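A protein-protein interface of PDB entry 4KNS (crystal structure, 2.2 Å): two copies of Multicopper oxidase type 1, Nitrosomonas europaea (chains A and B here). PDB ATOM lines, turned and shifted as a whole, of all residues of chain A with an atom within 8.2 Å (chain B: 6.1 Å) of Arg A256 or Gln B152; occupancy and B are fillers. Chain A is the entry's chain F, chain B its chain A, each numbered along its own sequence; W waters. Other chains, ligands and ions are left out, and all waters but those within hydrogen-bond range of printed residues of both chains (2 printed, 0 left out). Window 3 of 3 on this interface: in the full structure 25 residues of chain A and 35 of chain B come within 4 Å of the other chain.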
ATOM      1  N   ASN A 153     -19.960  32.843 -33.294  1.00  0.00           N
ATOM      2  CA  ASN A 153     -20.262  31.800 -32.306  1.00  0.00           C
ATOM      3  C   ASN A 153     -21.525  30.998 -32.646  1.00  0.00           C
ATOM      4  O   ASN A 153     -22.239  30.525 -31.757  1.00  0.00           O
ATOM      5  CB  ASN A 153     -20.331  32.391 -30.886  1.00  0.00           C
ATOM      6  CG  ASN A 153     -20.230  31.333 -29.801  1.00  0.00           C
ATOM      7  OD1 ASN A 153     -19.592  30.295 -29.978  1.00  0.00           O
ATOM      8  ND2 ASN A 153     -20.865  31.596 -28.666  1.00  0.00           N
ATOM      9  N   LYS A 154     -21.787  30.846 -33.942  1.00  0.00           N
ATOM     10  CA  LYS A 154     -22.967  30.128 -34.414  1.00  0.00           C
ATOM     11  C   LYS A 154     -22.645  28.664 -34.707  1.00  0.00           C
ATOM     12  O   LYS A 154     -22.393  28.283 -35.853  1.00  0.00           O
ATOM     13  CB  LYS A 154     -23.580  30.824 -35.634  1.00  0.00           C
ATOM     14  CG  LYS A 154     -24.314  32.112 -35.298  1.00  0.00           C
ATOM     15  CD  LYS A 154     -24.816  32.809 -36.552  1.00  0.00           C
ATOM     16  CE  LYS A 154     -25.541  34.101 -36.213  1.00  0.00           C
ATOM     17  NZ  LYS A 154     -26.030  34.795 -37.436  1.00  0.00           N
ATOM     18  N   TRP A 155     -22.648  27.858 -33.647  1.00  0.00           N
ATOM     19  CA  TRP A 155     -22.366  26.427 -33.736  1.00  0.00           C
ATOM     20  C   TRP A 155     -23.620  25.614 -33.852  1.00  0.00           C
ATOM     21  O   TRP A 155     -24.706  26.081 -33.501  1.00  0.00           O
ATOM     22  CB  TRP A 155     -21.552  25.971 -32.528  1.00  0.00           C
ATOM     23  CG  TRP A 155     -22.055  26.521 -31.214  1.00  0.00           C
ATOM     24  CD1 TRP A 155     -21.563  27.618 -30.512  1.00  0.00           C
ATOM     25  CD2 TRP A 155     -23.175  26.021 -30.402  1.00  0.00           C
ATOM     26  NE1 TRP A 155     -22.275  27.820 -29.357  1.00  0.00           N
ATOM     27  CE2 TRP A 155     -23.254  26.900 -29.229  1.00  0.00           C
ATOM     28  CE3 TRP A 155     -24.079  24.971 -30.520  1.00  0.00           C
ATOM     29  CZ2 TRP A 155     -24.205  26.716 -28.236  1.00  0.00           C
ATOM     30  CZ3 TRP A 155     -25.036  24.798 -29.512  1.00  0.00           C
ATOM     31  CH2 TRP A 155     -25.096  25.651 -28.399  1.00  0.00           C
ATOM     32  N   SER A 156     -23.474  24.387 -34.355  1.00  0.00           N
ATOM     33  CA  SER A 156     -24.596  23.466 -34.507  1.00  0.00           C
ATOM     34  C   SER A 156     -24.748  22.583 -33.274  1.00  0.00           C
ATOM     35  O   SER A 156     -25.861  22.344 -32.804  1.00  0.00           O
ATOM     36  CB  SER A 156     -24.418  22.595 -35.754  1.00  0.00           C
ATOM     37  OG  SER A 156     -24.364  23.384 -36.929  1.00  0.00           O
ATOM     38  N   ASN A 157     -23.618  22.102 -32.759  1.00  0.00           N
ATOM     39  CA  ASN A 157     -23.595  21.209 -31.604  1.00  0.00           C
ATOM     40  C   ASN A 157     -22.411  21.491 -30.682  1.00  0.00           C
ATOM     41  O   ASN A 157     -21.370  21.986 -31.121  1.00  0.00           O
ATOM     42  CB  ASN A 157     -23.541  19.743 -32.061  1.00  0.00           C
ATOM     43  CG  ASN A 157     -24.674  19.375 -33.004  1.00  0.00           C
ATOM     44  OD1 ASN A 157     -25.810  19.163 -32.582  1.00  0.00           O
ATOM     45  ND2 ASN A 157     -24.361  19.287 -34.291  1.00  0.00           N
ATOM     46  N   VAL A 158     -22.588  21.181 -29.400  1.00  0.00           N
ATOM     47  CA  VAL A 158     -21.490  21.162 -28.433  1.00  0.00           C
ATOM     48  C   VAL A 158     -21.238  19.691 -28.111  1.00  0.00           C
ATOM     49  O   VAL A 158     -22.113  19.011 -27.573  1.00  0.00           O
ATOM     50  CB  VAL A 158     -21.834  21.957 -27.155  1.00  0.00           C
ATOM     51  CG1 VAL A 158     -20.676  21.923 -26.166  1.00  0.00           C
ATOM     52  CG2 VAL A 158     -22.196  23.395 -27.503  1.00  0.00           C
ATOM     53  N   PHE A 165     -23.760  13.447 -29.110  1.00  0.00           N
ATOM     54  CA  PHE A 165     -24.285  12.435 -28.177  1.00  0.00           C
ATOM     55  C   PHE A 165     -23.514  11.109 -28.238  1.00  0.00           C
ATOM     56  O   PHE A 165     -24.112  10.028 -28.185  1.00  0.00           O
ATOM     57  CB  PHE A 165     -25.786  12.188 -28.412  1.00  0.00           C
ATOM     58  CG  PHE A 165     -26.675  13.317 -27.965  1.00  0.00           C
ATOM     59  CD1 PHE A 165     -26.852  13.592 -26.612  1.00  0.00           C
ATOM     60  CD2 PHE A 165     -27.362  14.086 -28.897  1.00  0.00           C
ATOM     61  CE1 PHE A 165     -27.680  14.626 -26.200  1.00  0.00           C
ATOM     62  CE2 PHE A 165     -28.194  15.120 -28.492  1.00  0.00           C
ATOM     63  CZ  PHE A 165     -28.353  15.389 -27.141  1.00  0.00           C
ATOM     64  N   GLU A 198     -16.612  28.386 -26.726  1.00  0.00           N
ATOM     65  CA  GLU A 198     -17.539  28.224 -25.605  1.00  0.00           C
ATOM     66  C   GLU A 198     -16.933  27.760 -24.282  1.00  0.00           C
ATOM     67  O   GLU A 198     -15.866  27.143 -24.234  1.00  0.00           O
ATOM     68  CB  GLU A 198     -18.720  27.322 -25.994  1.00  0.00           C
ATOM     69  CG  GLU A 198     -19.786  28.013 -26.831  1.00  0.00           C
ATOM     70  CD  GLU A 198     -20.673  28.952 -26.026  1.00  0.00           C
ATOM     71  OE1 GLU A 198     -20.447  29.123 -24.804  1.00  0.00           O
ATOM     72  OE2 GLU A 198     -21.611  29.523 -26.621  1.00  0.00           O
ATOM     73  N   ASP A 252     -22.415  19.345 -19.648  1.00  0.00           N
ATOM     74  CA  ASP A 252     -22.174  20.778 -19.618  1.00  0.00           C
ATOM     75  C   ASP A 252     -23.512  21.368 -19.181  1.00  0.00           C
ATOM     76  O   ASP A 252     -24.487  21.326 -19.932  1.00  0.00           O
ATOM     77  CB  ASP A 252     -21.771  21.286 -21.006  1.00  0.00           C
ATOM     78  CG  ASP A 252     -21.381  22.766 -21.016  1.00  0.00           C
ATOM     79  OD1 ASP A 252     -21.736  23.514 -20.077  1.00  0.00           O
ATOM     80  OD2 ASP A 252     -20.713  23.185 -21.985  1.00  0.00           O
ATOM     81  N   HIS A 253     -23.559  21.904 -17.963  1.00  0.00           N
ATOM     82  CA  HIS A 253     -24.829  22.291 -17.345  1.00  0.00           C
ATOM     83  C   HIS A 253     -25.455  23.537 -17.922  1.00  0.00           C
ATOM     84  O   HIS A 253     -26.583  23.884 -17.575  1.00  0.00           O
ATOM     85  CB  HIS A 253     -24.698  22.391 -15.828  1.00  0.00           C
ATOM     86  CG  HIS A 253     -25.945  21.977 -15.085  1.00  0.00           C
ATOM     87  ND1 HIS A 253     -27.111  22.633 -15.207  1.00  0.00           N
ATOM     88  CD2 HIS A 253     -26.174  20.931 -14.194  1.00  0.00           C
ATOM     89  CE1 HIS A 253     -28.042  22.042 -14.435  1.00  0.00           C
ATOM     90  NE2 HIS A 253     -27.467  21.000 -13.816  1.00  0.00           N
ATOM     91  N   SER A 254     -24.732  24.226 -18.804  1.00  0.00           N
ATOM     92  CA  SER A 254     -25.351  25.226 -19.662  1.00  0.00           C
ATOM     93  C   SER A 254     -26.245  24.450 -20.627  1.00  0.00           C
ATOM     94  O   SER A 254     -25.766  23.899 -21.620  1.00  0.00           O
ATOM     95  CB  SER A 254     -24.294  26.040 -20.411  1.00  0.00           C
ATOM     96  OG  SER A 254     -24.901  27.054 -21.188  1.00  0.00           O
ATOM     97  N   MET A 255     -27.539  24.398 -20.314  1.00  0.00           N
ATOM     98  CA  MET A 255     -28.455  23.416 -20.915  1.00  0.00           C
ATOM     99  C   MET A 255     -28.529  23.399 -22.446  1.00  0.00           C
ATOM    100  O   MET A 255     -28.773  22.345 -23.034  1.00  0.00           O
ATOM    101  CB  MET A 255     -29.862  23.514 -20.308  1.00  0.00           C
ATOM    102  CG  MET A 255     -29.996  22.950 -18.895  1.00  0.00           C
ATOM    103  SD  MET A 255     -29.202  21.354 -18.571  1.00  0.00           S
ATOM    104  CE  MET A 255     -29.922  20.304 -19.833  1.00  0.00           C
ATOM    105  N   ARG A 256     -28.319  24.549 -23.079  1.00  0.00           N
ATOM    106  CA  ARG A 256     -28.306  24.635 -24.543  1.00  0.00           C
ATOM    107  C   ARG A 256     -27.155  23.826 -25.153  1.00  0.00           C
ATOM    108  O   ARG A 256     -27.270  23.323 -26.275  1.00  0.00           O
ATOM    109  CB  ARG A 256     -28.271  26.098 -25.014  1.00  0.00           C
ATOM    110  CG  ARG A 256     -27.033  26.885 -24.603  1.00  0.00           C
ATOM    111  CD  ARG A 256     -27.203  28.381 -24.826  1.00  0.00           C
ATOM    112  NE  ARG A 256     -27.441  28.720 -26.227  1.00  0.00           N
ATOM    113  CZ  ARG A 256     -26.537  29.251 -27.045  1.00  0.00           C
ATOM    114  NH1 ARG A 256     -25.310  29.522 -26.617  1.00  0.00           N
ATOM    115  NH2 ARG A 256     -26.866  29.519 -28.299  1.00  0.00           N
ATOM    116  N   HIS A 257     -26.059  23.702 -24.405  1.00  0.00           N
ATOM    117  CA  HIS A 257     -24.916  22.877 -24.796  1.00  0.00           C
ATOM    118  C   HIS A 257     -25.244  21.418 -24.653  1.00  0.00           C
ATOM    119  O   HIS A 257     -24.989  20.628 -25.565  1.00  0.00           O
ATOM    120  CB  HIS A 257     -23.692  23.213 -23.944  1.00  0.00           C
ATOM    121  CG  HIS A 257     -23.183  24.627 -24.119  1.00  0.00           C
ATOM    122  ND1 HIS A 257     -21.985  25.021 -23.657  1.00  0.00           N
ATOM    123  CD2 HIS A 257     -23.750  25.740 -24.739  1.00  0.00           C
ATOM    124  CE1 HIS A 257     -21.795  26.320 -23.953  1.00  0.00           C
ATOM    125  NE2 HIS A 257     -22.876  26.757 -24.619  1.00  0.00           N
ATOM    126  N   ALA A 258     -25.813  21.057 -23.500  1.00  0.00           N
ATOM    127  CA  ALA A 258     -26.182  19.674 -23.193  1.00  0.00           C
ATOM    128  C   ALA A 258     -27.231  19.127 -24.158  1.00  0.00           C
ATOM    129  O   ALA A 258     -27.143  17.975 -24.587  1.00  0.00           O
ATOM    130  CB  ALA A 258     -26.671  19.560 -21.756  1.00  0.00           C
ATOM    131  N   HIS A 259     -28.213  19.961 -24.496  1.00  0.00           N
ATOM    132  CA  HIS A 259     -29.283  19.585 -25.422  1.00  0.00           C
ATOM    133  C   HIS A 259     -28.783  19.417 -26.836  1.00  0.00           C
ATOM    134  O   HIS A 259     -29.382  18.684 -27.627  1.00  0.00           O
ATOM    135  CB  HIS A 259     -30.407  20.617 -25.372  1.00  0.00           C
ATOM    136  CG  HIS A 259     -31.684  20.172 -26.051  1.00  0.00           C
ATOM    137  ND1 HIS A 259     -32.630  19.452 -25.416  1.00  0.00           N
ATOM    138  CD2 HIS A 259     -32.150  20.375 -27.350  1.00  0.00           C
ATOM    139  CE1 HIS A 259     -33.647  19.205 -26.264  1.00  0.00           C
ATOM    140  NE2 HIS A 259     -33.352  19.773 -27.446  1.00  0.00           N
ATOM    141  N   SER A 260     -27.679  20.090 -27.163  1.00  0.00           N
ATOM    142  CA  SER A 260     -27.075  19.995 -28.495  1.00  0.00           C
ATOM    143  C   SER A 260     -26.121  18.799 -28.637  1.00  0.00           C
ATOM    144  O   SER A 260     -25.635  18.518 -29.733  1.00  0.00           O
ATOM    145  CB  SER A 260     -26.373  21.306 -28.876  1.00  0.00           C
ATOM    146  OG  SER A 260     -25.167  21.485 -28.152  1.00  0.00           O
ATOM    147  N   GLY A 261     -25.853  18.103 -27.532  1.00  0.00           N
ATOM    148  CA  GLY A 261     -25.071  16.867 -27.581  1.00  0.00           C
ATOM    149  C   GLY A 261     -23.977  16.684 -26.545  1.00  0.00           C
ATOM    150  O   GLY A 261     -23.211  15.726 -26.626  1.00  0.00           O
ATOM    151  N   ALA A 262     -23.902  17.587 -25.568  1.00  0.00           N
ATOM    152  CA  ALA A 262     -22.854  17.531 -24.546  1.00  0.00           C
ATOM    153  C   ALA A 262     -23.278  16.739 -23.302  1.00  0.00           C
ATOM    154  O   ALA A 262     -23.285  17.267 -22.187  1.00  0.00           O
ATOM    155  CB  ALA A 262     -22.398  18.936 -24.170  1.00  0.00           C
ATOM    156  N   ILE B 105     -33.960  22.196 -20.237  1.00  0.00           N
ATOM    157  CA  ILE B 105     -33.872  23.628 -20.520  1.00  0.00           C
ATOM    158  C   ILE B 105     -35.204  24.358 -20.294  1.00  0.00           C
ATOM    159  O   ILE B 105     -35.227  25.434 -19.695  1.00  0.00           O
ATOM    160  CB  ILE B 105     -33.303  23.890 -21.942  1.00  0.00           C
ATOM    161  CG1 ILE B 105     -33.150  25.392 -22.203  1.00  0.00           C
ATOM    162  CG2 ILE B 105     -34.148  23.209 -23.017  1.00  0.00           C
ATOM    163  CD1 ILE B 105     -32.078  25.737 -23.214  1.00  0.00           C
ATOM    164  N   LYS B 147     -39.324  26.762 -27.355  1.00  0.00           N
ATOM    165  CA  LYS B 147     -38.098  26.045 -27.003  1.00  0.00           C
ATOM    166  C   LYS B 147     -36.897  26.455 -27.857  1.00  0.00           C
ATOM    167  O   LYS B 147     -35.748  26.285 -27.440  1.00  0.00           O
ATOM    168  CB  LYS B 147     -38.320  24.534 -27.091  1.00  0.00           C
ATOM    169  CG  LYS B 147     -39.206  23.978 -25.987  1.00  0.00           C
ATOM    170  CD  LYS B 147     -39.500  22.497 -26.178  1.00  0.00           C
ATOM    171  CE  LYS B 147     -40.633  22.264 -27.167  1.00  0.00           C
ATOM    172  NZ  LYS B 147     -41.051  20.836 -27.181  1.00  0.00           N
ATOM    173  N   THR B 148     -37.171  26.991 -29.044  1.00  0.00           N
ATOM    174  CA  THR B 148     -36.129  27.433 -29.973  1.00  0.00           C
ATOM    175  C   THR B 148     -35.394  28.667 -29.448  1.00  0.00           C
ATOM    176  O   THR B 148     -34.173  28.768 -29.579  1.00  0.00           O
ATOM    177  CB  THR B 148     -36.712  27.702 -31.378  1.00  0.00           C
ATOM    178  OG1 THR B 148     -37.332  26.508 -31.868  1.00  0.00           O
ATOM    179  CG2 THR B 148     -35.625  28.132 -32.362  1.00  0.00           C
ATOM    180  N   ALA B 149     -36.141  29.592 -28.850  1.00  0.00           N
ATOM    181  CA  ALA B 149     -35.564  30.799 -28.260  1.00  0.00           C
ATOM    182  C   ALA B 149     -34.647  30.473 -27.077  1.00  0.00           C
ATOM    183  O   ALA B 149     -33.618  31.124 -26.884  1.00  0.00           O
ATOM    184  CB  ALA B 149     -36.663  31.761 -27.837  1.00  0.00           C
ATOM    185  N   MET B 150     -35.026  29.459 -26.300  1.00  0.00           N
ATOM    186  CA  MET B 150     -34.220  28.993 -25.168  1.00  0.00           C
ATOM    187  C   MET B 150     -32.914  28.366 -25.645  1.00  0.00           C
ATOM    188  O   MET B 150     -31.857  28.590 -25.048  1.00  0.00           O
ATOM    189  CB  MET B 150     -35.008  27.997 -24.311  1.00  0.00           C
ATOM    190  CG  MET B 150     -36.235  28.584 -23.631  1.00  0.00           C
ATOM    191  SD  MET B 150     -37.288  27.315 -22.901  1.00  0.00           S
ATOM    192  CE  MET B 150     -38.599  28.313 -22.196  1.00  0.00           C
ATOM    193  N   MET B 151     -32.997  27.591 -26.724  1.00  0.00           N
ATOM    194  CA  MET B 151     -31.826  26.980 -27.354  1.00  0.00           C
ATOM    195  C   MET B 151     -30.884  28.030 -27.941  1.00  0.00           C
ATOM    196  O   MET B 151     -29.662  27.855 -27.927  1.00  0.00           O
ATOM    197  CB  MET B 151     -32.253  25.992 -28.445  1.00  0.00           C
ATOM    198  CG  MET B 151     -32.824  24.679 -27.924  1.00  0.00           C
ATOM    199  SD  MET B 151     -31.707  23.792 -26.816  1.00  0.00           S
ATOM    200  CE  MET B 151     -30.308  23.471 -27.893  1.00  0.00           C
ATOM    201  N   GLN B 152     -31.466  29.117 -28.446  1.00  0.00           N
ATOM    202  CA  GLN B 152     -30.709  30.228 -29.021  1.00  0.00           C
ATOM    203  C   GLN B 152     -30.299  31.271 -27.976  1.00  0.00           C
ATOM    204  O   GLN B 152     -29.701  32.295 -28.317  1.00  0.00           O
ATOM    205  CB  GLN B 152     -31.503  30.889 -30.153  1.00  0.00           C
ATOM    206  CG  GLN B 152     -31.683  30.012 -31.386  1.00  0.00           C
ATOM    207  CD  GLN B 152     -32.400  30.727 -32.518  1.00  0.00           C
ATOM    208  OE1 GLN B 152     -33.323  31.512 -32.294  1.00  0.00           O
ATOM    209  NE2 GLN B 152     -31.978  30.452 -33.747  1.00  0.00           N
ATOM    210  N   ASN B 153     -30.623  30.996 -26.710  1.00  0.00           N
ATOM    211  CA  ASN B 153     -30.252  31.846 -25.568  1.00  0.00           C
ATOM    212  C   ASN B 153     -30.838  33.262 -25.652  1.00  0.00           C
ATOM    213  O   ASN B 153     -30.229  34.236 -25.203  1.00  0.00           O
ATOM    214  CB  ASN B 153     -28.723  31.874 -25.384  1.00  0.00           C
ATOM    215  CG  ASN B 153     -28.301  32.371 -24.013  1.00  0.00           C
ATOM    216  OD1 ASN B 153     -28.982  32.139 -23.016  1.00  0.00           O
ATOM    217  ND2 ASN B 153     -27.167  33.060 -23.959  1.00  0.00           N
ATOM    218  N   LYS B 154     -32.034  33.362 -26.225  1.00  0.00           N
ATOM    219  CA  LYS B 154     -32.689  34.649 -26.418  1.00  0.00           C
ATOM    220  C   LYS B 154     -33.673  34.930 -25.289  1.00  0.00           C
ATOM    221  O   LYS B 154     -34.890  34.962 -25.493  1.00  0.00           O
ATOM    222  CB  LYS B 154     -33.371  34.708 -27.788  1.00  0.00           C
ATOM    223  CG  LYS B 154     -32.405  34.584 -28.956  1.00  0.00           C
ATOM    224  CD  LYS B 154     -33.127  34.672 -30.289  1.00  0.00           C
ATOM    225  CE  LYS B 154     -32.142  34.619 -31.445  1.00  0.00           C
ATOM    226  NZ  LYS B 154     -32.833  34.788 -32.754  1.00  0.00           N
ATOM    227  N   PRO B 196     -31.184  28.385 -17.308  1.00  0.00           N
ATOM    228  CA  PRO B 196     -30.455  27.181 -17.740  1.00  0.00           C
ATOM    229  C   PRO B 196     -29.145  27.389 -18.511  1.00  0.00           C
ATOM    230  O   PRO B 196     -28.355  26.448 -18.613  1.00  0.00           O
ATOM    231  CB  PRO B 196     -31.473  26.470 -18.641  1.00  0.00           C
ATOM    232  CG  PRO B 196     -32.333  27.566 -19.167  1.00  0.00           C
ATOM    233  CD  PRO B 196     -32.458  28.541 -18.036  1.00  0.00           C
ATOM    234  N   ASN B 197     -28.908  28.589 -19.036  1.00  0.00           N
ATOM    235  CA  ASN B 197     -27.781  28.802 -19.954  1.00  0.00           C
ATOM    236  C   ASN B 197     -26.652  29.701 -19.452  1.00  0.00           C
ATOM    237  O   ASN B 197     -25.480  29.438 -19.728  1.00  0.00           O
ATOM    238  CB  ASN B 197     -28.275  29.344 -21.303  1.00  0.00           C
ATOM    239  CG  ASN B 197     -29.316  28.453 -21.955  1.00  0.00           C
ATOM    240  OD1 ASN B 197     -29.220  27.225 -21.921  1.00  0.00           O
ATOM    241  ND2 ASN B 197     -30.314  29.074 -22.567  1.00  0.00           N
HETATM  242  O   HOH W   1     -32.099  20.445 -22.423  1.00  0.00           O
HETATM  243  O   HOH W   2     -28.886  24.829 -15.837  1.00  0.00           O
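Ser A254 touches Pro B196.
CB of Ile B105 touches CB of Met A255, at 3.8 Å.
OD1 of Asn B197 touches N of Met A255, at 3.7 Å.
Ile B105 touches Arg A256 (CD1 to N, 3.9 Å).
NH2 of Arg A256 touches C of Gln B152, 3.9 Å away.
Arg A256 touches Asn B153 (NE to CB, 3.5 Å).
His A259 touches Met B151.
Water W2 bridges a ring nitrogen (ND1) of His A253 and the backbone carbonyl oxygen (O) of Pro B196.
Water W1 lies within hydrogen-bond range of ND1 of His A259 and N of Ile B105.
Of the 11 printed residues of chain B, 6 touch a printed residue of chain A.
Printed residues of chain B that touch a printed residue of chain A: Ile B105, Met B151, Gln B152, Asn B153, Pro B196 and Asn B197.
Hydrophobic or aromatic side chains of chain B that line the printed part of chain A: Ile B105, Met B151 and Pro B196.
Printed residues of chain A that touch a printed residue of chain B: His A253, Ser A254, Met A255, Arg A256 and His A259.
Hydrophobic or aromatic side chains of chain A within 4 Å of the printed part of chain B: Met A255 and His A259.
Among the printed residues, 12 pairs touch across the chains.
Among the printed residues, no Asp or Glu carboxylate lies within 4 Å of a Lys or Arg side-chain nitrogen of the other chain.
Of the printed residues of chain B, His A253 touches Pro B196 (3.3 Å).
Of the printed residues of chain B, Met A255 touches Ile B105 (3.8 Å), Pro B196 (2.8 Å) and Asn B197 (3.7 Å).
Of chain B, only Ile B105, Met B151, Gln B152, Asn B153 and Asn B197 come within 4 Å of Arg A256.
Of the printed residues of chain B, His A259 touches Met B151.
Ser A260 touches none of the printed residues of chain B.
Of the printed residues of chain A, Met B151 touches Arg A256 (2.9 Å) and His A259 (3.5 Å).
Of chain A, only Arg A256 comes within 4 Å of Gln B152.
Of the printed residues of chain A, Asn B153 touches Arg A256.
The nearest residue of chain A that does not touch Gln B152 is Trp A155 (7.3 Å).
2 positions are printed for both chains.
Of the 12 pairs that touch across the chains among the printed residues, none has its exchanged pair printed and touching as well.
The backbone NH (N) of Met A255 sits at hydrogen-bond distance from the backbone carbonyl oxygen (O) of Pro B196 (2.8 Å).
O of Pro B196 sits close to O of His A253 (3.3 Å).
The side-chain amide oxygen of Asn B197 is in hydrogen-bond range of the backbone NH of Arg A256.
O of Asn B197 lies within hydrogen-bond range of OG of Ser A254.
The guanidinium group (NE) of Arg A256 is in hydrogen-bond range of the backbone carbonyl oxygen (O) of Met B151.
OE2 of Glu A198 lies within salt-bridge range of NH1 of Arg A256 (3.7 Å).
O of Arg A256 lies within hydrogen-bond range of OG of Ser A260, 3.4 Å away.
ND2 of Asn B197 lies close to OD1 of Asn B153, at 3.4 Å.
The backbone NH (N) of Ser A254 sits close to the side-chain carboxylate (OD1) of Asp A252 (3.3 Å).
OE1 of Gln B152 sits at hydrogen-bond distance from NZ of Lys B154 (3.3 Å).
The side-chain amide nitrogen of Asn B197 lies within hydrogen-bond range of the backbone carbonyl oxygen of Met B150 (3.0 Å).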
